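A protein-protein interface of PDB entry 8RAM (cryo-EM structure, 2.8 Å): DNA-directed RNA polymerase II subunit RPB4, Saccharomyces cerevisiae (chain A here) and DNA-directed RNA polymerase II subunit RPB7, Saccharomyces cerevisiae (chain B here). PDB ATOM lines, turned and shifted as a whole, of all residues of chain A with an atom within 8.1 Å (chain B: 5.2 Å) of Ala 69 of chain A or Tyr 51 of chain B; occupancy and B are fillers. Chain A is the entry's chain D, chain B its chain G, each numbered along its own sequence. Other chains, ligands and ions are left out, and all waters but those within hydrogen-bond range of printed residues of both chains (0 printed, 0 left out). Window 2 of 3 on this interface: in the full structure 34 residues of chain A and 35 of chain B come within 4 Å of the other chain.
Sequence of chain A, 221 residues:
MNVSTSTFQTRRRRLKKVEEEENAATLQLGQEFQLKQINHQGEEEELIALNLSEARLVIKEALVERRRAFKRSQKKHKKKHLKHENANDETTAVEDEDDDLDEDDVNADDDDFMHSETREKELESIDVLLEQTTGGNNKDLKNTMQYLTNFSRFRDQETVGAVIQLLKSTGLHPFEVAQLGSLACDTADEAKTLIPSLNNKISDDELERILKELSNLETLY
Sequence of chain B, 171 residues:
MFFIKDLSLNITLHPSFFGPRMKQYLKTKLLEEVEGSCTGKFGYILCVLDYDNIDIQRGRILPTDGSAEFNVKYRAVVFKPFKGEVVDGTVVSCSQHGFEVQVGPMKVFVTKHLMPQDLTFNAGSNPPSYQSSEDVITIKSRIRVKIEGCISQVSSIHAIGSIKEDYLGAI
Of the printed residues of chain B, Thr 134 of chain A touches Leu 31 (3.8 Å).
Of the printed residues of chain A, Leu 49 of chain B touches Ala 62 (3.8 Å).
Tyr 51 of chain B touches just one residue of chain A: Ala 69 (3.3 Å).
The side-chain carboxylate (OD1) of Asp 52 of chain B sits close to the side-chain carboxylate (OE1) of Glu 65 of chain A (2.8 Å).
NH1 of Arg 72 of chain A is in salt-bridge range of OD2 of Asp 52 of chain B (3.5 Å).
OG of Ser 73 of chain A lies within hydrogen-bond range of O of Ala 69 of chain A.
The guanidinium group (NH1) of Arg 68 of chain A is in salt-bridge range of the side-chain carboxylate (OE2) of Glu 65 of chain A (3.8 Å).
Among the printed residues, pairs that only touch across the chains: Ala 69 of chain A with Tyr 51 of chain B (3.3 Å), Thr 134 of chain A with Leu 31 of chain B (3.8 Å) and Ala 62 of chain A with Leu 49 of chain B (3.8 Å).
Of the 17 printed residues of chain A, 5 touch a printed residue of chain B.
Of the 9 printed residues of chain B, 4 touch a printed residue of chain A.
Among the printed residues, 5 pairs touch across the chains.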
ATOM      1  N   GLU A  61       6.044  -9.553  -2.474  1.00  0.00           N
ATOM      2  CA  GLU A  61       5.554 -10.616  -1.602  1.00  0.00           C
ATOM      3  C   GLU A  61       4.203 -10.250  -0.999  1.00  0.00           C
ATOM      4  O   GLU A  61       3.298 -11.091  -0.927  1.00  0.00           O
ATOM      5  CB  GLU A  61       6.573 -10.903  -0.501  1.00  0.00           C
ATOM      6  CG  GLU A  61       7.852 -11.558  -0.996  1.00  0.00           C
ATOM      7  CD  GLU A  61       8.863 -11.775   0.112  1.00  0.00           C
ATOM      8  OE1 GLU A  61       8.567 -11.411   1.270  1.00  0.00           O
ATOM      9  OE2 GLU A  61       9.955 -12.310  -0.173  1.00  0.00           O
ATOM     10  N   ALA A  62       4.048  -9.000  -0.559  1.00  0.00           N
ATOM     11  CA  ALA A  62       2.772  -8.565  -0.004  1.00  0.00           C
ATOM     12  C   ALA A  62       1.668  -8.625  -1.051  1.00  0.00           C
ATOM     13  O   ALA A  62       0.543  -9.046  -0.757  1.00  0.00           O
ATOM     14  CB  ALA A  62       2.900  -7.151   0.559  1.00  0.00           C
ATOM     15  N   LEU A  63       1.968  -8.200  -2.281  1.00  0.00           N
ATOM     16  CA  LEU A  63       0.970  -8.266  -3.345  1.00  0.00           C
ATOM     17  C   LEU A  63       0.575  -9.708  -3.640  1.00  0.00           C
ATOM     18  O   LEU A  63      -0.606 -10.005  -3.853  1.00  0.00           O
ATOM     19  CB  LEU A  63       1.501  -7.585  -4.608  1.00  0.00           C
ATOM     20  CG  LEU A  63       1.159  -6.104  -4.797  1.00  0.00           C
ATOM     21  CD1 LEU A  63      -0.343  -5.908  -4.956  1.00  0.00           C
ATOM     22  CD2 LEU A  63       1.690  -5.256  -3.649  1.00  0.00           C
ATOM     23  N   VAL A  64       1.552 -10.618  -3.660  1.00  0.00           N
ATOM     24  CA  VAL A  64       1.247 -12.027  -3.894  1.00  0.00           C
ATOM     25  C   VAL A  64       0.373 -12.574  -2.774  1.00  0.00           C
ATOM     26  O   VAL A  64      -0.580 -13.323  -3.019  1.00  0.00           O
ATOM     27  CB  VAL A  64       2.550 -12.837  -4.042  1.00  0.00           C
ATOM     28  CG1 VAL A  64       2.252 -14.330  -4.044  1.00  0.00           C
ATOM     29  CG2 VAL A  64       3.280 -12.438  -5.316  1.00  0.00           C
ATOM     30  N   GLU A  65       0.689 -12.219  -1.526  1.00  0.00           N
ATOM     31  CA  GLU A  65      -0.124 -12.676  -0.403  1.00  0.00           C
ATOM     32  C   GLU A  65      -1.549 -12.146  -0.503  1.00  0.00           C
ATOM     33  O   GLU A  65      -2.512 -12.880  -0.252  1.00  0.00           O
ATOM     34  CB  GLU A  65       0.517 -12.247   0.917  1.00  0.00           C
ATOM     35  CG  GLU A  65       1.829 -12.949   1.230  1.00  0.00           C
ATOM     36  CD  GLU A  65       1.650 -14.430   1.504  1.00  0.00           C
ATOM     37  OE1 GLU A  65       0.490 -14.885   1.593  1.00  0.00           O
ATOM     38  OE2 GLU A  65       2.671 -15.140   1.630  1.00  0.00           O
ATOM     39  N   ARG A  66      -1.704 -10.871  -0.866  1.00  0.00           N
ATOM     40  CA  ARG A  66      -3.040 -10.306  -1.029  1.00  0.00           C
ATOM     41  C   ARG A  66      -3.802 -11.015  -2.139  1.00  0.00           C
ATOM     42  O   ARG A  66      -4.996 -11.307  -1.996  1.00  0.00           O
ATOM     43  CB  ARG A  66      -2.946  -8.809  -1.321  1.00  0.00           C
ATOM     44  CG  ARG A  66      -2.352  -7.983  -0.193  1.00  0.00           C
ATOM     45  CD  ARG A  66      -2.041  -6.570  -0.659  1.00  0.00           C
ATOM     46  NE  ARG A  66      -1.204  -5.845   0.291  1.00  0.00           N
ATOM     47  CZ  ARG A  66      -0.732  -4.618   0.090  1.00  0.00           C
ATOM     48  NH1 ARG A  66      -1.015  -3.967  -1.032  1.00  0.00           N
ATOM     49  NH2 ARG A  66       0.026  -4.039   1.010  1.00  0.00           N
ATOM     50  N   ARG A  67      -3.132 -11.291  -3.261  1.00  0.00           N
ATOM     51  CA  ARG A  67      -3.788 -11.988  -4.360  1.00  0.00           C
ATOM     52  C   ARG A  67      -4.231 -13.381  -3.935  1.00  0.00           C
ATOM     53  O   ARG A  67      -5.343 -13.814  -4.262  1.00  0.00           O
ATOM     54  CB  ARG A  67      -2.849 -12.068  -5.563  1.00  0.00           C
ATOM     55  CG  ARG A  67      -3.466 -12.715  -6.795  1.00  0.00           C
ATOM     56  CD  ARG A  67      -2.474 -12.780  -7.945  1.00  0.00           C
ATOM     57  NE  ARG A  67      -1.304 -13.589  -7.615  1.00  0.00           N
ATOM     58  CZ  ARG A  67      -0.288 -13.811  -8.443  1.00  0.00           C
ATOM     59  NH1 ARG A  67      -0.289 -13.285  -9.661  1.00  0.00           N
ATOM     60  NH2 ARG A  67       0.733 -14.561  -8.052  1.00  0.00           N
ATOM     61  N   ARG A  68      -3.375 -14.099  -3.206  1.00  0.00           N
ATOM     62  CA  ARG A  68      -3.746 -15.425  -2.722  1.00  0.00           C
ATOM     63  C   ARG A  68      -4.932 -15.348  -1.768  1.00  0.00           C
ATOM     64  O   ARG A  68      -5.844 -16.181  -1.831  1.00  0.00           O
ATOM     65  CB  ARG A  68      -2.549 -16.086  -2.039  1.00  0.00           C
ATOM     66  CG  ARG A  68      -1.404 -16.420  -2.980  1.00  0.00           C
ATOM     67  CD  ARG A  68      -0.171 -16.874  -2.215  1.00  0.00           C
ATOM     68  NE  ARG A  68      -0.438 -18.045  -1.384  1.00  0.00           N
ATOM     69  CZ  ARG A  68       0.459 -18.623  -0.593  1.00  0.00           C
ATOM     70  NH1 ARG A  68       1.695 -18.143  -0.518  1.00  0.00           N
ATOM     71  NH2 ARG A  68       0.123 -19.686   0.127  1.00  0.00           N
ATOM     72  N   ALA A  69      -4.929 -14.360  -0.870  1.00  0.00           N
ATOM     73  CA  ALA A  69      -6.038 -14.204   0.064  1.00  0.00           C
ATOM     74  C   ALA A  69      -7.342 -13.941  -0.678  1.00  0.00           C
ATOM     75  O   ALA A  69      -8.379 -14.544  -0.375  1.00  0.00           O
ATOM     76  CB  ALA A  69      -5.738 -13.072   1.046  1.00  0.00           C
ATOM     77  N   PHE A  70      -7.306 -13.043  -1.665  1.00  0.00           N
ATOM     78  CA  PHE A  70      -8.508 -12.755  -2.440  1.00  0.00           C
ATOM     79  C   PHE A  70      -8.976 -13.986  -3.205  1.00  0.00           C
ATOM     80  O   PHE A  70     -10.178 -14.269  -3.266  1.00  0.00           O
ATOM     81  CB  PHE A  70      -8.255 -11.593  -3.401  1.00  0.00           C
ATOM     82  CG  PHE A  70      -8.369 -10.238  -2.757  1.00  0.00           C
ATOM     83  CD1 PHE A  70      -9.606  -9.738  -2.385  1.00  0.00           C
ATOM     84  CD2 PHE A  70      -7.243  -9.464  -2.533  1.00  0.00           C
ATOM     85  CE1 PHE A  70      -9.716  -8.493  -1.794  1.00  0.00           C
ATOM     86  CE2 PHE A  70      -7.349  -8.218  -1.944  1.00  0.00           C
ATOM     87  CZ  PHE A  70      -8.586  -7.733  -1.574  1.00  0.00           C
ATOM     88  N   LYS A  71      -8.041 -14.735  -3.793  1.00  0.00           N
ATOM     89  CA  LYS A  71      -8.414 -15.924  -4.551  1.00  0.00           C
ATOM     90  C   LYS A  71      -9.079 -16.959  -3.653  1.00  0.00           C
ATOM     91  O   LYS A  71     -10.112 -17.535  -4.010  1.00  0.00           O
ATOM     92  CB  LYS A  71      -7.178 -16.515  -5.232  1.00  0.00           C
ATOM     93  CG  LYS A  71      -7.466 -17.749  -6.077  1.00  0.00           C
ATOM     94  CD  LYS A  71      -6.230 -18.216  -6.839  1.00  0.00           C
ATOM     95  CE  LYS A  71      -5.120 -18.678  -5.906  1.00  0.00           C
ATOM     96  NZ  LYS A  71      -5.558 -19.777  -5.001  1.00  0.00           N
ATOM     97  N   ARG A  72      -8.503 -17.206  -2.474  1.00  0.00           N
ATOM     98  CA  ARG A  72      -9.089 -18.193  -1.572  1.00  0.00           C
ATOM     99  C   ARG A  72     -10.439 -17.724  -1.045  1.00  0.00           C
ATOM    100  O   ARG A  72     -11.366 -18.531  -0.901  1.00  0.00           O
ATOM    101  CB  ARG A  72      -8.132 -18.500  -0.419  1.00  0.00           C
ATOM    102  CG  ARG A  72      -7.824 -17.319   0.476  1.00  0.00           C
ATOM    103  CD  ARG A  72      -6.884 -17.705   1.607  1.00  0.00           C
ATOM    104  NE  ARG A  72      -5.596 -18.183   1.114  1.00  0.00           N
ATOM    105  CZ  ARG A  72      -4.594 -18.583   1.893  1.00  0.00           C
ATOM    106  NH1 ARG A  72      -4.725 -18.565   3.213  1.00  0.00           N
ATOM    107  NH2 ARG A  72      -3.459 -19.001   1.350  1.00  0.00           N
ATOM    108  N   SER A  73     -10.575 -16.429  -0.751  1.00  0.00           N
ATOM    109  CA  SER A  73     -11.858 -15.918  -0.278  1.00  0.00           C
ATOM    110  C   SER A  73     -12.931 -16.048  -1.352  1.00  0.00           C
ATOM    111  O   SER A  73     -14.076 -16.407  -1.053  1.00  0.00           O
ATOM    112  CB  SER A  73     -11.712 -14.461   0.160  1.00  0.00           C
ATOM    113  OG  SER A  73     -11.340 -13.637  -0.929  1.00  0.00           O
ATOM    114  N   GLN A  74     -12.580 -15.761  -2.608  1.00  0.00           N
ATOM    115  CA  GLN A  74     -13.561 -15.845  -3.684  1.00  0.00           C
ATOM    116  C   GLN A  74     -13.875 -17.291  -4.046  1.00  0.00           C
ATOM    117  O   GLN A  74     -14.979 -17.581  -4.523  1.00  0.00           O
ATOM    118  CB  GLN A  74     -13.055 -15.088  -4.912  1.00  0.00           C
ATOM    119  CG  GLN A  74     -14.044 -15.029  -6.069  1.00  0.00           C
ATOM    120  CD  GLN A  74     -15.312 -14.274  -5.718  1.00  0.00           C
ATOM    121  OE1 GLN A  74     -15.394 -13.624  -4.677  1.00  0.00           O
ATOM    122  NE2 GLN A  74     -16.310 -14.356  -6.590  1.00  0.00           N
ATOM    123  N   LYS A  75     -12.928 -18.207  -3.833  1.00  0.00           N
ATOM    124  CA  LYS A  75     -13.173 -19.607  -4.165  1.00  0.00           C
ATOM    125  C   LYS A  75     -14.319 -20.176  -3.338  1.00  0.00           C
ATOM    126  O   LYS A  75     -15.175 -20.897  -3.864  1.00  0.00           O
ATOM    127  CB  LYS A  75     -11.898 -20.424  -3.949  1.00  0.00           C
ATOM    128  CG  LYS A  75     -12.021 -21.886  -4.351  1.00  0.00           C
ATOM    129  CD  LYS A  75     -10.705 -22.623  -4.168  1.00  0.00           C
ATOM    130  CE  LYS A  75     -10.823 -24.081  -4.583  1.00  0.00           C
ATOM    131  NZ  LYS A  75      -9.539 -24.816  -4.413  1.00  0.00           N
ATOM    132  N   THR A 133      -5.527  -6.182  -7.598  1.00  0.00           N
ATOM    133  CA  THR A 133      -5.680  -6.079  -6.152  1.00  0.00           C
ATOM    134  C   THR A 133      -5.168  -4.724  -5.691  1.00  0.00           C
ATOM    135  O   THR A 133      -4.072  -4.305  -6.079  1.00  0.00           O
ATOM    136  CB  THR A 133      -4.930  -7.205  -5.427  1.00  0.00           C
ATOM    137  OG1 THR A 133      -5.015  -7.004  -4.010  1.00  0.00           O
ATOM    138  CG2 THR A 133      -3.465  -7.245  -5.847  1.00  0.00           C
ATOM    139  N   THR A 134      -5.957  -4.047  -4.856  1.00  0.00           N
ATOM    140  CA  THR A 134      -5.619  -2.707  -4.375  1.00  0.00           C
ATOM    141  C   THR A 134      -5.416  -1.746  -5.544  1.00  0.00           C
ATOM    142  O   THR A 134      -4.533  -0.885  -5.520  1.00  0.00           O
ATOM    143  CB  THR A 134      -4.379  -2.735  -3.478  1.00  0.00           C
ATOM    144  OG1 THR A 134      -3.246  -3.192  -4.229  1.00  0.00           O
ATOM    145  CG2 THR A 134      -4.600  -3.654  -2.286  1.00  0.00           C
ATOM    146  N   LYS B  27     -10.511  -6.316   6.940  1.00  0.00           N
ATOM    147  CA  LYS B  27      -9.295  -6.230   6.140  1.00  0.00           C
ATOM    148  C   LYS B  27      -9.468  -5.262   4.976  1.00  0.00           C
ATOM    149  O   LYS B  27      -8.551  -4.499   4.653  1.00  0.00           O
ATOM    150  CB  LYS B  27      -8.904  -7.617   5.629  1.00  0.00           C
ATOM    151  CG  LYS B  27      -8.501  -8.597   6.723  1.00  0.00           C
ATOM    152  CD  LYS B  27      -7.199  -8.190   7.397  1.00  0.00           C
ATOM    153  CE  LYS B  27      -6.795  -9.186   8.472  1.00  0.00           C
ATOM    154  NZ  LYS B  27      -6.548 -10.546   7.919  1.00  0.00           N
ATOM    155  N   THR B  28     -10.635  -5.283   4.327  1.00  0.00           N
ATOM    156  CA  THR B  28     -10.876  -4.353   3.229  1.00  0.00           C
ATOM    157  C   THR B  28     -10.840  -2.910   3.716  1.00  0.00           C
ATOM    158  O   THR B  28     -10.260  -2.038   3.057  1.00  0.00           O
ATOM    159  CB  THR B  28     -12.218  -4.655   2.562  1.00  0.00           C
ATOM    160  OG1 THR B  28     -13.250  -4.705   3.555  1.00  0.00           O
ATOM    161  CG2 THR B  28     -12.162  -5.979   1.815  1.00  0.00           C
ATOM    162  N   LEU B  31      -7.255  -1.929   4.355  1.00  0.00           N
ATOM    163  CA  LEU B  31      -6.579  -1.626   3.097  1.00  0.00           C
ATOM    164  C   LEU B  31      -6.995  -0.260   2.565  1.00  0.00           C
ATOM    165  O   LEU B  31      -6.152   0.519   2.108  1.00  0.00           O
ATOM    166  CB  LEU B  31      -6.872  -2.715   2.065  1.00  0.00           C
ATOM    167  CG  LEU B  31      -5.867  -3.867   1.982  1.00  0.00           C
ATOM    168  CD1 LEU B  31      -5.749  -4.608   3.306  1.00  0.00           C
ATOM    169  CD2 LEU B  31      -6.259  -4.828   0.869  1.00  0.00           C
ATOM    170  N   LEU B  49       2.740  -5.233   4.676  1.00  0.00           N
ATOM    171  CA  LEU B  49       3.166  -6.578   4.323  1.00  0.00           C
ATOM    172  C   LEU B  49       2.596  -7.594   5.306  1.00  0.00           C
ATOM    173  O   LEU B  49       2.045  -7.247   6.355  1.00  0.00           O
ATOM    174  CB  LEU B  49       4.697  -6.667   4.280  1.00  0.00           C
ATOM    175  CG  LEU B  49       5.480  -5.999   5.415  1.00  0.00           C
ATOM    176  CD1 LEU B  49       5.239  -6.689   6.749  1.00  0.00           C
ATOM    177  CD2 LEU B  49       6.965  -5.977   5.085  1.00  0.00           C
ATOM    178  N   ASP B  50       2.740  -8.870   4.947  1.00  0.00           N
ATOM    179  CA  ASP B  50       2.255  -9.982   5.761  1.00  0.00           C
ATOM    180  C   ASP B  50       0.745  -9.875   5.981  1.00  0.00           C
ATOM    181  O   ASP B  50       0.250  -9.834   7.108  1.00  0.00           O
ATOM    182  CB  ASP B  50       3.005 -10.046   7.096  1.00  0.00           C
ATOM    183  CG  ASP B  50       4.493 -10.272   6.917  1.00  0.00           C
ATOM    184  OD1 ASP B  50       4.886 -10.882   5.901  1.00  0.00           O
ATOM    185  OD2 ASP B  50       5.271  -9.842   7.795  1.00  0.00           O
ATOM    186  N   TYR B  51       0.014  -9.833   4.864  1.00  0.00           N
ATOM    187  CA  TYR B  51      -1.438  -9.709   4.933  1.00  0.00           C
ATOM    188  C   TYR B  51      -2.066 -10.912   5.626  1.00  0.00           C
ATOM    189  O   TYR B  51      -2.978 -10.760   6.446  1.00  0.00           O
ATOM    190  CB  TYR B  51      -2.014  -9.541   3.526  1.00  0.00           C
ATOM    191  CG  TYR B  51      -3.523  -9.471   3.483  1.00  0.00           C
ATOM    192  CD1 TYR B  51      -4.284 -10.615   3.280  1.00  0.00           C
ATOM    193  CD2 TYR B  51      -4.187  -8.263   3.644  1.00  0.00           C
ATOM    194  CE1 TYR B  51      -5.664 -10.557   3.238  1.00  0.00           C
ATOM    195  CE2 TYR B  51      -5.566  -8.195   3.603  1.00  0.00           C
ATOM    196  CZ  TYR B  51      -6.299  -9.344   3.401  1.00  0.00           C
ATOM    197  OH  TYR B  51      -7.673  -9.282   3.360  1.00  0.00           O
ATOM    198  N   ASP B  52      -1.594 -12.119   5.307  1.00  0.00           N
ATOM    199  CA  ASP B  52      -2.164 -13.321   5.904  1.00  0.00           C
ATOM    200  C   ASP B  52      -1.809 -13.463   7.378  1.00  0.00           C
ATOM    201  O   ASP B  52      -2.530 -14.146   8.111  1.00  0.00           O
ATOM    202  CB  ASP B  52      -1.693 -14.560   5.140  1.00  0.00           C
ATOM    203  CG  ASP B  52      -2.194 -14.588   3.710  1.00  0.00           C
ATOM    204  OD1 ASP B  52      -1.745 -13.746   2.904  1.00  0.00           O
ATOM    205  OD2 ASP B  52      -3.037 -15.452   3.391  1.00  0.00           O
ATOM    206  N   ASN B  53      -0.724 -12.836   7.827  1.00  0.00           N
ATOM    207  CA  ASN B  53      -0.284 -12.937   9.212  1.00  0.00           C
ATOM    208  C   ASN B  53      -0.804 -11.800  10.083  1.00  0.00           C
ATOM    209  O   ASN B  53      -0.440 -11.726  11.261  1.00  0.00           O
ATOM    210  CB  ASN B  53       1.248 -12.971   9.272  1.00  0.00           C
ATOM    211  CG  ASN B  53       1.771 -13.373  10.638  1.00  0.00           C
ATOM    212  OD1 ASN B  53       1.057 -13.984  11.433  1.00  0.00           O
ATOM    213  ND2 ASN B  53       3.022 -13.030  10.916  1.00  0.00           N
ATOM    214  N   ILE B  54      -1.646 -10.918   9.541  1.00  0.00           N
ATOM    215  CA  ILE B  54      -2.172  -9.813  10.332  1.00  0.00           C
ATOM    216  C   ILE B  54      -2.970 -10.367  11.502  1.00  0.00           C
ATOM    217  O   ILE B  54      -3.897 -11.166  11.323  1.00  0.00           O
ATOM    218  CB  ILE B  54      -3.033  -8.887   9.460  1.00  0.00           C
ATOM    219  CG1 ILE B  54      -2.208  -8.298   8.310  1.00  0.00           C
ATOM    220  CG2 ILE B  54      -3.643  -7.775  10.303  1.00  0.00           C
ATOM    221  CD1 ILE B  54      -1.004  -7.487   8.753  1.00  0.00           C
